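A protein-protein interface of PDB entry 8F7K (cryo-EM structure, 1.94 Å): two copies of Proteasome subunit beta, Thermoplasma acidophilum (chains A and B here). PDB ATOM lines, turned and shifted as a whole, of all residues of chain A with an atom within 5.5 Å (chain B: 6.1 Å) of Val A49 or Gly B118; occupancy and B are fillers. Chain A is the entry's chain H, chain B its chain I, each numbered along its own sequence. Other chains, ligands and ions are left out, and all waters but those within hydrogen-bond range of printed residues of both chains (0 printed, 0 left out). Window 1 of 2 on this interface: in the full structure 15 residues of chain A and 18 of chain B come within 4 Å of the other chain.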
ATOM      1  N   VAL A  20     -24.987   1.793  11.423  1.00  0.00           N
ATOM      2  CA  VAL A  20     -25.378   1.099  10.160  1.00  0.00           C
ATOM      3  C   VAL A  20     -26.375  -0.026  10.466  1.00  0.00           C
ATOM      4  O   VAL A  20     -26.051  -0.894  11.261  1.00  0.00           O
ATOM      5  CB  VAL A  20     -24.163   0.610   9.345  1.00  0.00           C
ATOM      6  CG1 VAL A  20     -24.575  -0.071   8.049  1.00  0.00           C
ATOM      7  CG2 VAL A  20     -23.146   1.709   9.095  1.00  0.00           C
ATOM      8  N   MET A  22     -27.931  -3.118   9.068  1.00  0.00           N
ATOM      9  CA  MET A  22     -27.843  -4.204   8.036  1.00  0.00           C
ATOM     10  C   MET A  22     -28.653  -5.417   8.542  1.00  0.00           C
ATOM     11  O   MET A  22     -28.446  -5.785   9.701  1.00  0.00           O
ATOM     12  CB  MET A  22     -26.352  -4.520   7.833  1.00  0.00           C
ATOM     13  CG  MET A  22     -25.839  -4.828   6.441  1.00  0.00           C
ATOM     14  SD  MET A  22     -24.182  -5.596   6.574  1.00  0.00           S
ATOM     15  CE  MET A  22     -23.143  -4.368   5.785  1.00  0.00           C
ATOM     16  N   GLY A  47     -28.361   6.165   2.560  1.00  0.00           N
ATOM     17  CA  GLY A  47     -29.084   5.213   1.742  1.00  0.00           C
ATOM     18  C   GLY A  47     -28.390   3.861   1.711  1.00  0.00           C
ATOM     19  O   GLY A  47     -27.818   3.414   2.712  1.00  0.00           O
ATOM     20  N   LEU A  48     -28.452   3.216   0.548  1.00  0.00           N
ATOM     21  CA  LEU A  48     -27.864   1.892   0.382  1.00  0.00           C
ATOM     22  C   LEU A  48     -26.345   1.982   0.482  1.00  0.00           C
ATOM     23  O   LEU A  48     -25.713   2.769  -0.231  1.00  0.00           O
ATOM     24  CB  LEU A  48     -28.284   1.293  -0.957  1.00  0.00           C
ATOM     25  CG  LEU A  48     -27.910  -0.169  -1.206  1.00  0.00           C
ATOM     26  CD1 LEU A  48     -28.565  -1.075  -0.174  1.00  0.00           C
ATOM     27  CD2 LEU A  48     -28.295  -0.592  -2.614  1.00  0.00           C
ATOM     28  N   VAL A  49     -25.762   1.173   1.370  1.00  0.00           N
ATOM     29  CA  VAL A  49     -24.327   1.253   1.633  1.00  0.00           C
ATOM     30  C   VAL A  49     -23.526   0.880   0.391  1.00  0.00           C
ATOM     31  O   VAL A  49     -22.532   1.536   0.057  1.00  0.00           O
ATOM     32  CB  VAL A  49     -23.956   0.363   2.834  1.00  0.00           C
ATOM     33  CG1 VAL A  49     -22.456   0.392   3.082  1.00  0.00           C
ATOM     34  CG2 VAL A  49     -24.712   0.810   4.076  1.00  0.00           C
ATOM     35  N   GLY A  50     -23.940  -0.178  -0.310  1.00  0.00           N
ATOM     36  CA  GLY A  50     -23.190  -0.619  -1.475  1.00  0.00           C
ATOM     37  C   GLY A  50     -23.137   0.426  -2.573  1.00  0.00           C
ATOM     38  O   GLY A  50     -22.076   0.701  -3.136  1.00  0.00           O
ATOM     39  N   ASP A  51     -24.286   1.030  -2.885  1.00  0.00           N
ATOM     40  CA  ASP A  51     -24.325   2.067  -3.913  1.00  0.00           C
ATOM     41  C   ASP A  51     -23.493   3.277  -3.502  1.00  0.00           C
ATOM     42  O   ASP A  51     -22.762   3.849  -4.319  1.00  0.00           O
ATOM     43  CB  ASP A  51     -25.770   2.481  -4.189  1.00  0.00           C
ATOM     44  CG  ASP A  51     -26.551   1.417  -4.932  1.00  0.00           C
ATOM     45  OD1 ASP A  51     -25.948   0.398  -5.324  1.00  0.00           O
ATOM     46  OD2 ASP A  51     -27.772   1.601  -5.124  1.00  0.00           O
ATOM     47  N   ALA A  52     -23.597   3.680  -2.235  1.00  0.00           N
ATOM     48  CA  ALA A  52     -22.887   4.865  -1.770  1.00  0.00           C
ATOM     49  C   ALA A  52     -21.376   4.674  -1.828  1.00  0.00           C
ATOM     50  O   ALA A  52     -20.647   5.582  -2.241  1.00  0.00           O
ATOM     51  CB  ALA A  52     -23.332   5.214  -0.351  1.00  0.00           C
ATOM     52  N   GLN A  53     -20.886   3.501  -1.419  1.00  0.00           N
ATOM     53  CA  GLN A  53     -19.446   3.266  -1.401  1.00  0.00           C
ATOM     54  C   GLN A  53     -18.865   3.248  -2.811  1.00  0.00           C
ATOM     55  O   GLN A  53     -17.744   3.720  -3.031  1.00  0.00           O
ATOM     56  CB  GLN A  53     -19.136   1.963  -0.667  1.00  0.00           C
ATOM     57  CG  GLN A  53     -19.399   2.031   0.830  1.00  0.00           C
ATOM     58  CD  GLN A  53     -19.147   0.713   1.536  1.00  0.00           C
ATOM     59  OE1 GLN A  53     -19.066  -0.340   0.905  1.00  0.00           O
ATOM     60  NE2 GLN A  53     -19.020   0.767   2.857  1.00  0.00           N
ATOM     61  N   VAL A  54     -19.609   2.702  -3.776  1.00  0.00           N
ATOM     62  CA  VAL A  54     -19.153   2.711  -5.164  1.00  0.00           C
ATOM     63  C   VAL A  54     -19.040   4.142  -5.679  1.00  0.00           C
ATOM     64  O   VAL A  54     -18.070   4.498  -6.359  1.00  0.00           O
ATOM     65  CB  VAL A  54     -20.093   1.862  -6.041  1.00  0.00           C
ATOM     66  CG1 VAL A  54     -19.738   2.017  -7.510  1.00  0.00           C
ATOM     67  CG2 VAL A  54     -20.023   0.401  -5.632  1.00  0.00           C
ATOM     68  N   SER B  84     -16.807  -6.155  -2.872  1.00  0.00           N
ATOM     69  CA  SER B  84     -17.837  -5.122  -2.900  1.00  0.00           C
ATOM     70  C   SER B  84     -18.185  -4.731  -4.331  1.00  0.00           C
ATOM     71  O   SER B  84     -19.363  -4.583  -4.677  1.00  0.00           O
ATOM     72  CB  SER B  84     -17.366  -3.904  -2.104  1.00  0.00           C
ATOM     73  OG  SER B  84     -18.323  -2.862  -2.142  1.00  0.00           O
ATOM     74  N   ASN B  88     -21.885  -5.481  -6.211  1.00  0.00           N
ATOM     75  CA  ASN B  88     -22.673  -4.307  -6.574  1.00  0.00           C
ATOM     76  C   ASN B  88     -22.923  -4.230  -8.075  1.00  0.00           C
ATOM     77  O   ASN B  88     -23.943  -3.679  -8.504  1.00  0.00           O
ATOM     78  CB  ASN B  88     -21.979  -3.036  -6.084  1.00  0.00           C
ATOM     79  CG  ASN B  88     -22.838  -1.797  -6.262  1.00  0.00           C
ATOM     80  OD1 ASN B  88     -22.708  -1.077  -7.250  1.00  0.00           O
ATOM     81  ND2 ASN B  88     -23.724  -1.550  -5.305  1.00  0.00           N
ATOM     82  N   SER B 112     -17.567  -7.268   6.980  1.00  0.00           N
ATOM     83  CA  SER B 112     -18.886  -7.813   6.694  1.00  0.00           C
ATOM     84  C   SER B 112     -19.383  -7.237   5.377  1.00  0.00           C
ATOM     85  O   SER B 112     -19.398  -6.016   5.197  1.00  0.00           O
ATOM     86  CB  SER B 112     -19.869  -7.492   7.821  1.00  0.00           C
ATOM     87  OG  SER B 112     -21.172  -7.941   7.499  1.00  0.00           O
ATOM     88  N   ILE B 113     -19.788  -8.113   4.460  1.00  0.00           N
ATOM     89  CA  ILE B 113     -20.219  -7.714   3.126  1.00  0.00           C
ATOM     90  C   ILE B 113     -21.605  -8.286   2.870  1.00  0.00           C
ATOM     91  O   ILE B 113     -21.838  -9.481   3.080  1.00  0.00           O
ATOM     92  CB  ILE B 113     -19.229  -8.185   2.043  1.00  0.00           C
ATOM     93  CG1 ILE B 113     -17.799  -7.795   2.426  1.00  0.00           C
ATOM     94  CG2 ILE B 113     -19.593  -7.587   0.697  1.00  0.00           C
ATOM     95  CD1 ILE B 113     -16.754  -8.264   1.446  1.00  0.00           C
ATOM     96  N   ASP B 114     -22.521  -7.435   2.414  1.00  0.00           N
ATOM     97  CA  ASP B 114     -23.888  -7.832   2.124  1.00  0.00           C
ATOM     98  C   ASP B 114     -24.057  -8.091   0.627  1.00  0.00           C
ATOM     99  O   ASP B 114     -23.129  -7.931  -0.169  1.00  0.00           O
ATOM    100  CB  ASP B 114     -24.875  -6.770   2.618  1.00  0.00           C
ATOM    101  CG  ASP B 114     -24.598  -5.399   2.032  1.00  0.00           C
ATOM    102  OD1 ASP B 114     -24.862  -5.193   0.830  1.00  0.00           O
ATOM    103  OD2 ASP B 114     -24.115  -4.522   2.779  1.00  0.00           O
ATOM    104  N   ALA B 115     -25.271  -8.491   0.244  1.00  0.00           N
ATOM    105  CA  ALA B 115     -25.543  -8.868  -1.139  1.00  0.00           C
ATOM    106  C   ALA B 115     -25.449  -7.691  -2.103  1.00  0.00           C
ATOM    107  O   ALA B 115     -25.227  -7.906  -3.299  1.00  0.00           O
ATOM    108  CB  ALA B 115     -26.925  -9.513  -1.245  1.00  0.00           C
ATOM    109  N   ALA B 116     -25.616  -6.463  -1.621  1.00  0.00           N
ATOM    110  CA  ALA B 116     -25.567  -5.286  -2.475  1.00  0.00           C
ATOM    111  C   ALA B 116     -24.170  -4.689  -2.590  1.00  0.00           C
ATOM    112  O   ALA B 116     -24.004  -3.663  -3.256  1.00  0.00           O
ATOM    113  CB  ALA B 116     -26.539  -4.219  -1.961  1.00  0.00           C
ATOM    114  N   GLY B 117     -23.169  -5.301  -1.966  1.00  0.00           N
ATOM    115  CA  GLY B 117     -21.810  -4.814  -2.046  1.00  0.00           C
ATOM    116  C   GLY B 117     -21.388  -3.864  -0.948  1.00  0.00           C
ATOM    117  O   GLY B 117     -20.304  -3.279  -1.046  1.00  0.00           O
ATOM    118  N   GLY B 118     -22.204  -3.683   0.086  1.00  0.00           N
ATOM    119  CA  GLY B 118     -21.801  -2.834   1.198  1.00  0.00           C
ATOM    120  C   GLY B 118     -20.822  -3.562   2.101  1.00  0.00           C
ATOM    121  O   GLY B 118     -21.084  -4.686   2.547  1.00  0.00           O
ATOM    122  N   SER B 119     -19.687  -2.925   2.378  1.00  0.00           N
ATOM    123  CA  SER B 119     -18.620  -3.526   3.169  1.00  0.00           C
ATOM    124  C   SER B 119     -18.311  -2.623   4.354  1.00  0.00           C
ATOM    125  O   SER B 119     -18.029  -1.434   4.174  1.00  0.00           O
ATOM    126  CB  SER B 119     -17.365  -3.747   2.319  1.00  0.00           C
ATOM    127  OG  SER B 119     -16.310  -4.288   3.095  1.00  0.00           O
ATOM    128  N   VAL B 120     -18.362  -3.187   5.560  1.00  0.00           N
ATOM    129  CA  VAL B 120     -18.109  -2.450   6.793  1.00  0.00           C
ATOM    130  C   VAL B 120     -17.132  -3.246   7.646  1.00  0.00           C
ATOM    131  O   VAL B 120     -17.345  -4.440   7.889  1.00  0.00           O
ATOM    132  CB  VAL B 120     -19.408  -2.180   7.579  1.00  0.00           C
ATOM    133  CG1 VAL B 120     -19.109  -1.391   8.844  1.00  0.00           C
ATOM    134  CG2 VAL B 120     -20.421  -1.444   6.714  1.00  0.00           C
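OD1 of Asp A51 is in hydrogen-bond range of ND2 of Asn B88 (3.0 Å).
NE2 of Gln A53 lies within hydrogen-bond range of O of Ser B119 (2.7 Å).
The backbone carbonyl oxygen of Ala B116 lies within hydrogen-bond range of the side-chain amide nitrogen of Asn B88 (3.0 Å).
The backbone NH of Ser B112 sits at hydrogen-bond distance from the backbone carbonyl oxygen of Val B120 (3.0 Å).
OD1 of Asp B114 sits at hydrogen-bond distance from N of Ala B116.
The side-chain carboxylate (OD1) of Asp B114 sits at hydrogen-bond distance from the backbone NH (N) of Gly B118.
The side-chain carboxylate of Asp B114 sits at hydrogen-bond distance from the backbone NH of Gly B117.
Among the printed residues, pairs that only touch across the chains: Met A22 with Asp B114, Gly A50 with Asn B88, Val A54 with Asn B88, Gly A50 with Gly B118, Gly A50 with Ala B116, Gln A53 with Gly B118, Gln A53 with Gly B117, Gly A50 with Gly B117, Val A49 with Gly B118, Met A22 with Gly B118 and Met A22 with Ser B112.
Of chain B, only Gly B118 comes within 4 Å of Val A49.
Gly B118 touches four residues of chain A.
Of the printed residues of chain B, Gln A53 touches Gly B117 (3.7 Å), Gly B118 (3.7 Å) and Ser B119 (2.7 Å).
Of the printed residues of chain A, Asn B88 touches Gly A50 (3.4 Å), Asp A51 (3.0 Å) and Val A54 (3.5 Å).
Printed residues of chain B within 4 Å of Asp A51: Asn B88.
Of the printed residues of chain A, Ser B119 touches Gln A53.
Of the printed residues of chain B, Met A22 touches Ser B112, Asp B114 and Gly B118.
The nearest printed residue of chain A that does not touch Gly B118 is Asp A51 (5.9 Å).
Along chain B the printed residues that touch a printed residue of chain A span positions 88 to 119.
Of the 10 printed residues of chain A, 6 touch a printed residue of chain B.
Printed residues of chain A that touch a printed residue of chain B: Met A22, Val A49, Gly A50, Asp A51, Gln A53 and Val A54.
Among the printed residues, 13 pairs touch across the chains.
Among the printed residues, no Asp or Glu carboxylate lies within 4 Å of a Lys or Arg side-chain nitrogen of the other chain.
No position is printed for both chains.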
